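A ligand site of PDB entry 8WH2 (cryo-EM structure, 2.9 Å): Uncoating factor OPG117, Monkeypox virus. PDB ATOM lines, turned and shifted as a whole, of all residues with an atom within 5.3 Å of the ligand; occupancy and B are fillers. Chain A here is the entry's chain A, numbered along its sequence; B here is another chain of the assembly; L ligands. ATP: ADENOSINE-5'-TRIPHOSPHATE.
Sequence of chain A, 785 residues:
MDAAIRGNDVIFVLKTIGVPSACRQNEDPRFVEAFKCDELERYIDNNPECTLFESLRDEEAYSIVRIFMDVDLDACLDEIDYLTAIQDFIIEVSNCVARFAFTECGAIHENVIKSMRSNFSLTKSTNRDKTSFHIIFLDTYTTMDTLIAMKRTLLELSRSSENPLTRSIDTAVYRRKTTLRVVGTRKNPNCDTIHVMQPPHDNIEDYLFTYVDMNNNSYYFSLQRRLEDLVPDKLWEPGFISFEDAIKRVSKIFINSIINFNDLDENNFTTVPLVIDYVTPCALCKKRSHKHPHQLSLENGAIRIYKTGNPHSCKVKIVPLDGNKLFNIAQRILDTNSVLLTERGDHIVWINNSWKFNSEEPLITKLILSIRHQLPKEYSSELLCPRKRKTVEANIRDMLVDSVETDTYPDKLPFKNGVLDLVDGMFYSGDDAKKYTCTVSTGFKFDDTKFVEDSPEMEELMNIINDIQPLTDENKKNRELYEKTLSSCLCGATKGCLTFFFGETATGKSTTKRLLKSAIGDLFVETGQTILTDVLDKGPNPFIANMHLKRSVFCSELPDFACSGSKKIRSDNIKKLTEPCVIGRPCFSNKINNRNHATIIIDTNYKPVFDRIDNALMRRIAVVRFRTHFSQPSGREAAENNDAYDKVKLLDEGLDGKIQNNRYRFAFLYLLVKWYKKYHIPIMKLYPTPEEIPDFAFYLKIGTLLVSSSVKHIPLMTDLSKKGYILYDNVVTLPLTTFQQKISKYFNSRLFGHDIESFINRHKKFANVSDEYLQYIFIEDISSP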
ATOM      1  N   ASN A 463      -5.116  -1.849  15.142  1.00  0.00           N
ATOM      2  CA  ASN A 463      -4.640  -0.482  15.011  1.00  0.00           C
ATOM      3  C   ASN A 463      -5.002   0.347  16.245  1.00  0.00           C
ATOM      4  O   ASN A 463      -4.178   1.117  16.743  1.00  0.00           O
ATOM      5  CB  ASN A 463      -5.220   0.165  13.756  1.00  0.00           C
ATOM      6  CG  ASN A 463      -4.470  -0.236  12.494  1.00  0.00           C
ATOM      7  OD1 ASN A 463      -3.281  -0.547  12.537  1.00  0.00           O
ATOM      8  ND2 ASN A 463      -5.167  -0.233  11.364  1.00  0.00           N
ATOM      9  N   ILE A 464      -6.225   0.180  16.757  1.00  0.00           N
ATOM     10  CA  ILE A 464      -6.641   0.915  17.950  1.00  0.00           C
ATOM     11  C   ILE A 464      -5.776   0.543  19.152  1.00  0.00           C
ATOM     12  O   ILE A 464      -5.319   1.412  19.911  1.00  0.00           O
ATOM     13  CB  ILE A 464      -8.135   0.667  18.241  1.00  0.00           C
ATOM     14  CG1 ILE A 464      -9.001   1.253  17.135  1.00  0.00           C
ATOM     15  CG2 ILE A 464      -8.524   1.239  19.592  1.00  0.00           C
ATOM     16  CD1 ILE A 464     -10.369   0.631  17.045  1.00  0.00           C
ATOM     17  N   ASP A 467      -2.360   1.941  18.836  1.00  0.00           N
ATOM     18  CA  ASP A 467      -2.366   3.374  19.103  1.00  0.00           C
ATOM     19  C   ASP A 467      -2.382   3.649  20.605  1.00  0.00           C
ATOM     20  O   ASP A 467      -1.626   4.493  21.096  1.00  0.00           O
ATOM     21  CB  ASP A 467      -3.574   4.031  18.427  1.00  0.00           C
ATOM     22  CG  ASP A 467      -3.297   4.455  17.009  1.00  0.00           C
ATOM     23  OD1 ASP A 467      -2.139   4.842  16.715  1.00  0.00           O
ATOM     24  OD2 ASP A 467      -4.227   4.405  16.175  1.00  0.00           O
ATOM     25  N   ILE A 468      -3.235   2.929  21.339  1.00  0.00           N
ATOM     26  CA  ILE A 468      -3.362   3.178  22.774  1.00  0.00           C
ATOM     27  C   ILE A 468      -2.090   2.780  23.504  1.00  0.00           C
ATOM     28  O   ILE A 468      -1.550   3.545  24.319  1.00  0.00           O
ATOM     29  CB  ILE A 468      -4.597   2.467  23.342  1.00  0.00           C
ATOM     30  CG1 ILE A 468      -5.868   3.039  22.732  1.00  0.00           C
ATOM     31  CG2 ILE A 468      -4.632   2.578  24.858  1.00  0.00           C
ATOM     32  CD1 ILE A 468      -7.134   2.416  23.267  1.00  0.00           C
ATOM     33  N   GLU A 504      -2.913  10.867  31.852  1.00  0.00           N
ATOM     34  CA  GLU A 504      -3.512  12.180  31.683  1.00  0.00           C
ATOM     35  C   GLU A 504      -4.832  12.036  30.925  1.00  0.00           C
ATOM     36  O   GLU A 504      -5.328  10.937  30.705  1.00  0.00           O
ATOM     37  CB  GLU A 504      -2.536  13.130  30.991  1.00  0.00           C
ATOM     38  N   THR A 505      -5.419  13.161  30.515  1.00  0.00           N
ATOM     39  CA  THR A 505      -6.702  13.131  29.852  1.00  0.00           C
ATOM     40  C   THR A 505      -6.569  12.684  28.403  1.00  0.00           C
ATOM     41  O   THR A 505      -5.526  12.872  27.766  1.00  0.00           O
ATOM     42  CB  THR A 505      -7.379  14.507  29.917  1.00  0.00           C
ATOM     43  OG1 THR A 505      -8.767  14.380  29.580  1.00  0.00           O
ATOM     44  CG2 THR A 505      -6.705  15.493  28.977  1.00  0.00           C
ATOM     45  N   ALA A 506      -7.637  12.063  27.891  1.00  0.00           N
ATOM     46  CA  ALA A 506      -7.730  11.620  26.502  1.00  0.00           C
ATOM     47  C   ALA A 506      -6.549  10.731  26.118  1.00  0.00           C
ATOM     48  O   ALA A 506      -5.770  11.039  25.212  1.00  0.00           O
ATOM     49  CB  ALA A 506      -7.861  12.820  25.557  1.00  0.00           C
ATOM     50  N   THR A 507      -6.436   9.602  26.821  1.00  0.00           N
ATOM     51  CA  THR A 507      -5.345   8.666  26.582  1.00  0.00           C
ATOM     52  C   THR A 507      -5.800   7.257  26.243  1.00  0.00           C
ATOM     53  O   THR A 507      -4.946   6.430  25.889  1.00  0.00           O
ATOM     54  CB  THR A 507      -4.422   8.616  27.806  1.00  0.00           C
ATOM     55  OG1 THR A 507      -5.196   8.610  29.007  1.00  0.00           O
ATOM     56  CG2 THR A 507      -3.484   9.818  27.817  1.00  0.00           C
ATOM     57  N   GLY A 508      -7.090   6.950  26.335  1.00  0.00           N
ATOM     58  CA  GLY A 508      -7.607   5.653  25.939  1.00  0.00           C
ATOM     59  C   GLY A 508      -8.114   4.769  27.048  1.00  0.00           C
ATOM     60  O   GLY A 508      -8.504   3.620  26.764  1.00  0.00           O
ATOM     61  N   LYS A 509      -8.133   5.239  28.294  1.00  0.00           N
ATOM     62  CA  LYS A 509      -8.556   4.398  29.403  1.00  0.00           C
ATOM     63  C   LYS A 509     -10.045   4.042  29.309  1.00  0.00           C
ATOM     64  O   LYS A 509     -10.420   2.873  29.471  1.00  0.00           O
ATOM     65  CB  LYS A 509      -8.253   5.098  30.726  1.00  0.00           C
ATOM     66  CG  LYS A 509      -6.896   5.784  30.737  1.00  0.00           C
ATOM     67  CD  LYS A 509      -6.614   6.476  32.062  1.00  0.00           C
ATOM     68  CE  LYS A 509      -7.340   7.803  32.173  1.00  0.00           C
ATOM     69  NZ  LYS A 509      -6.551   8.914  31.578  1.00  0.00           N
ATOM     70  N   SER A 510     -10.897   5.026  29.041  1.00  0.00           N
ATOM     71  CA  SER A 510     -12.313   4.744  28.884  1.00  0.00           C
ATOM     72  C   SER A 510     -12.593   3.923  27.637  1.00  0.00           C
ATOM     73  O   SER A 510     -13.519   3.112  27.634  1.00  0.00           O
ATOM     74  CB  SER A 510     -13.128   6.037  28.868  1.00  0.00           C
ATOM     75  OG  SER A 510     -13.453   6.444  30.183  1.00  0.00           O
ATOM     76  N   THR A 511     -11.809   4.135  26.574  1.00  0.00           N
ATOM     77  CA  THR A 511     -11.947   3.292  25.390  1.00  0.00           C
ATOM     78  C   THR A 511     -11.644   1.836  25.721  1.00  0.00           C
ATOM     79  O   THR A 511     -12.363   0.918  25.294  1.00  0.00           O
ATOM     80  CB  THR A 511     -11.032   3.794  24.282  1.00  0.00           C
ATOM     81  OG1 THR A 511     -11.498   5.074  23.820  1.00  0.00           O
ATOM     82  CG2 THR A 511     -11.016   2.828  23.108  1.00  0.00           C
ATOM     83  N   ARG A 514     -14.602   0.426  27.748  1.00  0.00           N
ATOM     84  CA  ARG A 514     -15.765   0.132  26.921  1.00  0.00           C
ATOM     85  C   ARG A 514     -15.515  -1.079  26.033  1.00  0.00           C
ATOM     86  O   ARG A 514     -16.430  -1.889  25.820  1.00  0.00           O
ATOM     87  CB  ARG A 514     -16.121   1.367  26.080  1.00  0.00           C
ATOM     88  CG  ARG A 514     -16.583   2.553  26.909  1.00  0.00           C
ATOM     89  CD  ARG A 514     -17.422   3.524  26.094  1.00  0.00           C
ATOM     90  NE  ARG A 514     -16.608   4.568  25.486  1.00  0.00           N
ATOM     91  CZ  ARG A 514     -16.294   5.714  26.072  1.00  0.00           C
ATOM     92  NH1 ARG A 514     -16.717   6.001  27.283  1.00  0.00           N
ATOM     93  NH2 ARG A 514     -15.537   6.592  25.416  1.00  0.00           N
ATOM     94  N   GLU A 557     -12.507   7.651  38.237  1.00  0.00           N
ATOM     95  CA  GLU A 557     -12.439   9.048  38.666  1.00  0.00           C
ATOM     96  C   GLU A 557     -12.095   9.192  40.155  1.00  0.00           C
ATOM     97  O   GLU A 557     -12.890   9.679  40.961  1.00  0.00           O
ATOM     98  CB  GLU A 557     -13.736   9.785  38.323  1.00  0.00           C
ATOM     99  CG  GLU A 557     -14.399   9.369  37.009  1.00  0.00           C
ATOM    100  CD  GLU A 557     -13.534   9.597  35.784  1.00  0.00           C
ATOM    101  OE1 GLU A 557     -12.481  10.258  35.886  1.00  0.00           O
ATOM    102  OE2 GLU A 557     -13.911   9.107  34.699  1.00  0.00           O
ATOM    103  N   ASP A 603      -9.763   3.673  37.035  1.00  0.00           N
ATOM    104  CA  ASP A 603      -9.318   4.752  36.175  1.00  0.00           C
ATOM    105  C   ASP A 603      -9.028   5.991  37.009  1.00  0.00           C
ATOM    106  O   ASP A 603      -9.783   6.332  37.918  1.00  0.00           O
ATOM    107  CB  ASP A 603     -10.387   5.076  35.129  1.00  0.00           C
ATOM    108  CG  ASP A 603     -10.534   3.996  34.082  1.00  0.00           C
ATOM    109  OD1 ASP A 603      -9.653   3.118  34.017  1.00  0.00           O
ATOM    110  OD2 ASP A 603     -11.526   4.036  33.323  1.00  0.00           O
ATOM    111  N   ASN A 605      -6.690   9.994  36.925  1.00  0.00           N
ATOM    112  CA  ASN A 605      -5.662  10.943  36.520  1.00  0.00           C
ATOM    113  C   ASN A 605      -4.640  11.198  37.610  1.00  0.00           C
ATOM    114  O   ASN A 605      -3.627  11.851  37.356  1.00  0.00           O
ATOM    115  CB  ASN A 605      -6.310  12.284  36.116  1.00  0.00           C
ATOM    116  CG  ASN A 605      -7.308  12.134  34.986  1.00  0.00           C
ATOM    117  OD1 ASN A 605      -8.511  12.006  35.223  1.00  0.00           O
ATOM    118  ND2 ASN A 605      -6.822  12.173  33.762  1.00  0.00           N
ATOM    119  N   PHE A 630      -4.953  11.756  22.042  1.00  0.00           N
ATOM    120  CA  PHE A 630      -5.828  11.844  20.874  1.00  0.00           C
ATOM    121  C   PHE A 630      -6.537  13.193  20.945  1.00  0.00           C
ATOM    122  O   PHE A 630      -7.413  13.396  21.794  1.00  0.00           O
ATOM    123  CB  PHE A 630      -6.818  10.688  20.847  1.00  0.00           C
ATOM    124  CG  PHE A 630      -6.189   9.339  21.033  1.00  0.00           C
ATOM    125  CD1 PHE A 630      -5.465   8.763  20.011  1.00  0.00           C
ATOM    126  CD2 PHE A 630      -6.320   8.655  22.220  1.00  0.00           C
ATOM    127  CE1 PHE A 630      -4.872   7.519  20.176  1.00  0.00           C
ATOM    128  CE2 PHE A 630      -5.731   7.412  22.399  1.00  0.00           C
ATOM    129  CZ  PHE A 630      -5.009   6.853  21.376  1.00  0.00           C
ATOM    130  N   LYS A 649      -1.965  11.713  18.535  1.00  0.00           N
ATOM    131  CA  LYS A 649      -2.692  11.183  17.389  1.00  0.00           C
ATOM    132  C   LYS A 649      -3.968  11.982  17.176  1.00  0.00           C
ATOM    133  O   LYS A 649      -4.403  12.736  18.046  1.00  0.00           O
ATOM    134  CB  LYS A 649      -3.046   9.699  17.580  1.00  0.00           C
ATOM    135  CG  LYS A 649      -2.141   8.749  16.819  1.00  0.00           C
ATOM    136  CD  LYS A 649      -2.779   8.318  15.512  1.00  0.00           C
ATOM    137  CE  LYS A 649      -4.187   7.802  15.731  1.00  0.00           C
ATOM    138  NZ  LYS A 649      -4.819   7.305  14.479  1.00  0.00           N
ATOM    139  N   LEU A 650      -4.558  11.808  16.000  1.00  0.00           N
ATOM    140  CA  LEU A 650      -5.780  12.523  15.657  1.00  0.00           C
ATOM    141  C   LEU A 650      -6.999  11.796  16.223  1.00  0.00           C
ATOM    142  O   LEU A 650      -7.120  10.579  16.105  1.00  0.00           O
ATOM    143  CB  LEU A 650      -5.907  12.662  14.140  1.00  0.00           C
ATOM    144  CG  LEU A 650      -7.122  13.420  13.614  1.00  0.00           C
ATOM    145  CD1 LEU A 650      -6.960  14.915  13.868  1.00  0.00           C
ATOM    146  CD2 LEU A 650      -7.326  13.152  12.138  1.00  0.00           C
ATOM    147  N   LEU A 651      -7.890  12.554  16.861  1.00  0.00           N
ATOM    148  CA  LEU A 651      -9.074  11.985  17.477  1.00  0.00           C
ATOM    149  C   LEU A 651     -10.042  11.453  16.417  1.00  0.00           C
ATOM    150  O   LEU A 651     -10.192  12.039  15.329  1.00  0.00           O
ATOM    151  CB  LEU A 651      -9.777  13.032  18.344  1.00  0.00           C
ATOM    152  CG  LEU A 651     -10.847  12.570  19.319  1.00  0.00           C
ATOM    153  CD1 LEU A 651     -10.697  13.283  20.650  1.00  0.00           C
ATOM    154  CD2 LEU A 651     -12.239  12.796  18.751  1.00  0.00           C
ATOM    155  N   ASP A 652     -10.683  10.335  16.730  1.00  0.00           N
ATOM    156  CA  ASP A 652     -11.689   9.729  15.868  1.00  0.00           C
ATOM    157  C   ASP A 652     -13.054   9.939  16.498  1.00  0.00           C
ATOM    158  O   ASP A 652     -13.256   9.607  17.671  1.00  0.00           O
ATOM    159  CB  ASP A 652     -11.410   8.235  15.672  1.00  0.00           C
ATOM    160  CG  ASP A 652     -12.269   7.604  14.602  1.00  0.00           C
ATOM    161  OD1 ASP A 652     -13.154   8.295  14.054  1.00  0.00           O
ATOM    162  OD2 ASP A 652     -12.073   6.409  14.301  1.00  0.00           O
ATOM    163  N   LEU A 655     -15.600   6.495  16.677  1.00  0.00           N
ATOM    164  CA  LEU A 655     -15.121   5.312  17.389  1.00  0.00           C
ATOM    165  C   LEU A 655     -15.997   4.982  18.591  1.00  0.00           C
ATOM    166  O   LEU A 655     -16.243   3.817  18.885  1.00  0.00           O
ATOM    167  CB  LEU A 655     -13.670   5.509  17.822  1.00  0.00           C
ATOM    168  CG  LEU A 655     -12.985   4.303  18.468  1.00  0.00           C
ATOM    169  CD1 LEU A 655     -13.110   3.082  17.570  1.00  0.00           C
ATOM    170  CD2 LEU A 655     -11.540   4.602  18.772  1.00  0.00           C
ATOM    171  N   ASP A 656     -16.468   6.015  19.304  1.00  0.00           N
ATOM    172  CA  ASP A 656     -17.321   5.778  20.459  1.00  0.00           C
ATOM    173  C   ASP A 656     -18.608   5.064  20.057  1.00  0.00           C
ATOM    174  O   ASP A 656     -19.024   4.105  20.701  1.00  0.00           O
ATOM    175  CB  ASP A 656     -17.633   7.088  21.173  1.00  0.00           C
ATOM    176  CG  ASP A 656     -16.833   7.261  22.452  1.00  0.00           C
ATOM    177  OD1 ASP A 656     -16.764   8.396  22.962  1.00  0.00           O
ATOM    178  OD2 ASP A 656     -16.286   6.246  22.943  1.00  0.00           O
ATOM    179  N   GLU B 579     -19.901  10.388  32.075  1.00  0.00           N
ATOM    180  CA  GLU B 579     -19.805   8.988  31.715  1.00  0.00           C
ATOM    181  C   GLU B 579     -21.151   8.450  31.233  1.00  0.00           C
ATOM    182  O   GLU B 579     -22.207   8.945  31.627  1.00  0.00           O
ATOM    183  CB  GLU B 579     -19.346   8.168  32.926  1.00  0.00           C
ATOM    184  CG  GLU B 579     -17.889   8.374  33.302  1.00  0.00           C
ATOM    185  CD  GLU B 579     -16.953   8.258  32.122  1.00  0.00           C
ATOM    186  OE1 GLU B 579     -16.631   7.118  31.730  1.00  0.00           O
ATOM    187  OE2 GLU B 579     -16.540   9.298  31.577  1.00  0.00           O
ATOM    188  N   ARG B 619     -12.073  20.041  29.724  1.00  0.00           N
ATOM    189  CA  ARG B 619     -12.581  19.358  28.548  1.00  0.00           C
ATOM    190  C   ARG B 619     -14.090  19.135  28.592  1.00  0.00           C
ATOM    191  O   ARG B 619     -14.648  18.560  27.656  1.00  0.00           O
ATOM    192  CB  ARG B 619     -11.870  17.998  28.397  1.00  0.00           C
ATOM    193  CG  ARG B 619     -11.567  17.588  26.966  1.00  0.00           C
ATOM    194  CD  ARG B 619     -10.637  16.374  26.946  1.00  0.00           C
ATOM    195  NE  ARG B 619     -11.077  15.315  27.829  1.00  0.00           N
ATOM    196  CZ  ARG B 619     -11.652  14.187  27.433  1.00  0.00           C
ATOM    197  NH1 ARG B 619     -11.866  13.935  26.152  1.00  0.00           N
ATOM    198  NH2 ARG B 619     -12.003  13.279  28.344  1.00  0.00           N
ATOM    199  N   ARG B 620     -14.768  19.586  29.667  1.00  0.00           N
ATOM    200  CA  ARG B 620     -16.177  19.260  29.859  1.00  0.00           C
ATOM    201  C   ARG B 620     -16.989  20.459  30.331  1.00  0.00           C
ATOM    202  O   ARG B 620     -18.024  20.291  30.977  1.00  0.00           O
ATOM    203  CB  ARG B 620     -16.345  18.126  30.865  1.00  0.00           C
ATOM    204  CG  ARG B 620     -15.480  16.898  30.614  1.00  0.00           C
ATOM    205  CD  ARG B 620     -15.198  16.158  31.905  1.00  0.00           C
ATOM    206  NE  ARG B 620     -15.037  14.721  31.696  1.00  0.00           N
ATOM    207  CZ  ARG B 620     -13.942  14.156  31.235  1.00  0.00           C
ATOM    208  NH1 ARG B 620     -12.865  14.860  30.931  1.00  0.00           N
ATOM    209  NH2 ARG B 620     -13.910  12.831  31.075  1.00  0.00           N
HETATM  210  PG  ATP L   1     -11.688   8.881  30.893  1.00  0.00           P
HETATM  211  O1G ATP L   1     -13.153   8.831  30.628  1.00  0.00           O
HETATM  212  O2G ATP L   1     -11.179  10.266  31.322  1.00  0.00           O
HETATM  213  O3G ATP L   1     -11.215   7.831  31.908  1.00  0.00           O
HETATM  214  PB  ATP L   1      -9.791   9.219  28.597  1.00  0.00           P
HETATM  215  O1B ATP L   1     -10.074  10.656  28.418  1.00  0.00           O
HETATM  216  O2B ATP L   1      -8.415   8.873  29.120  1.00  0.00           O
HETATM  217  O3B ATP L   1     -10.860   8.548  29.563  1.00  0.00           O
HETATM  218  PA  ATP L   1     -11.080   8.361  26.074  1.00  0.00           P
HETATM  219  O1A ATP L   1     -12.460   8.545  26.583  1.00  0.00           O
HETATM  220  O2A ATP L   1     -10.851   7.068  25.300  1.00  0.00           O
HETATM  221  O3A ATP L   1     -10.017   8.398  27.248  1.00  0.00           O
HETATM  222  O5' ATP L   1     -10.655   9.568  25.153  1.00  0.00           O
HETATM  223  C5' ATP L   1      -9.996   9.354  23.890  1.00  0.00           C
HETATM  224  C4' ATP L   1     -10.802  10.011  22.784  1.00  0.00           C
HETATM  225  O4' ATP L   1     -10.223   9.678  21.509  1.00  0.00           O
HETATM  226  C3' ATP L   1     -12.246   9.548  22.683  1.00  0.00           C
HETATM  227  O3' ATP L   1     -13.054  10.540  22.053  1.00  0.00           O
HETATM  228  C2' ATP L   1     -12.122   8.286  21.828  1.00  0.00           C
HETATM  229  O2' ATP L   1     -13.311   8.040  21.087  1.00  0.00           O
HETATM  230  C1' ATP L   1     -10.956   8.632  20.897  1.00  0.00           C
HETATM  231  N9  ATP L   1     -10.046   7.515  20.664  1.00  0.00           N
HETATM  232  C8  ATP L   1      -9.742   6.496  21.520  1.00  0.00           C
HETATM  233  N7  ATP L   1      -8.887   5.627  21.043  1.00  0.00           N
HETATM  234  C5  ATP L   1      -8.597   6.114  19.781  1.00  0.00           C
HETATM  235  C6  ATP L   1      -7.752   5.648  18.754  1.00  0.00           C
HETATM  236  N6  ATP L   1      -7.014   4.537  18.846  1.00  0.00           N
HETATM  237  N1  ATP L   1      -7.693   6.368  17.611  1.00  0.00           N
HETATM  238  C2  ATP L   1      -8.441   7.477  17.509  1.00  0.00           C
HETATM  239  N3  ATP L   1      -9.272   8.007  18.413  1.00  0.00           N
HETATM  240  C4  ATP L   1      -9.300   7.277  19.528  1.00  0.00           C
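Merely in contact with the ligand: Leu 655, Asp 467, Glu 579 of chain B, Phe 630, Leu 650, Leu 651, Ile 464 and Asp 656.
Hydrophobic or aromatic side chains within 4 Å of the ligand: Ile 464, Phe 630, Leu 651 and Leu 655.
The nearest printed residue that does not touch the ligand is Glu 504 (4.04 Å).
The side-chain hydroxyl of Ser 510 sits at hydrogen-bond distance from an oxygen (O1G) of the ligand (2.4 Å).
N of Thr 511 lies within hydrogen-bond range of O2A of the ligand (3.3 Å).
O2A of the ligand lies within hydrogen-bond range of OG1 of Thr 511, 2.6 Å away.
N of Ala 506 is in hydrogen-bond range of O1B of the ligand, at 2.9 Å.
NZ of Lys 509 is in salt-bridge range of O2B of the ligand (3.1 Å).
The backbone NH (N) of Thr 507 is in hydrogen-bond range of an oxygen (O2B) of the ligand.
An oxygen (O2B) of the ligand is in hydrogen-bond range of the side-chain hydroxyl (OG1) of Thr 507 (3.2 Å).
N3 of the ligand is in hydrogen-bond range of N of Asp 652, 3.2 Å away.
The guanidinium group (NH2) of Arg 619 of chain B lies within salt-bridge range of an oxygen (O1B) of the ligand, at 3.3 Å.
The backbone NH of Gly 508 sits at hydrogen-bond distance from an oxygen (O3A) of the ligand (3.4 Å).
The guanidinium group (NH2) of Arg 620 of chain B lies within salt-bridge range of an oxygen (O2G) of the ligand (3.8 Å).
O1A of the ligand is in salt-bridge range of NH2 of Arg 514, 3.8 Å away.
The backbone NH (N) of Phe 630 lies within hydrogen-bond range of the backbone carbonyl oxygen (O) of Ala 506 (3.4 Å).
OG1 of Thr 507 sits at hydrogen-bond distance from NZ of Lys 509 (2.9 Å).
The side-chain amino group of Lys 509 is in hydrogen-bond range of the backbone carbonyl oxygen of Glu 504 (2.5 Å).
The backbone carbonyl oxygen (O) of Glu 504 lies within hydrogen-bond range of the side-chain hydroxyl (OG1) of Thr 507 (2.9 Å).
The guanidinium group (NE) of Arg 619 of chain B is in hydrogen-bond range of the side-chain hydroxyl (OG1) of Thr 505, 3.0 Å away.
OD2 of Asp 467 is in salt-bridge range of NZ of Lys 649 (3.4 Å).
OD2 of Asp 656 is in salt-bridge range of NH2 of Arg 514, 2.6 Å away.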
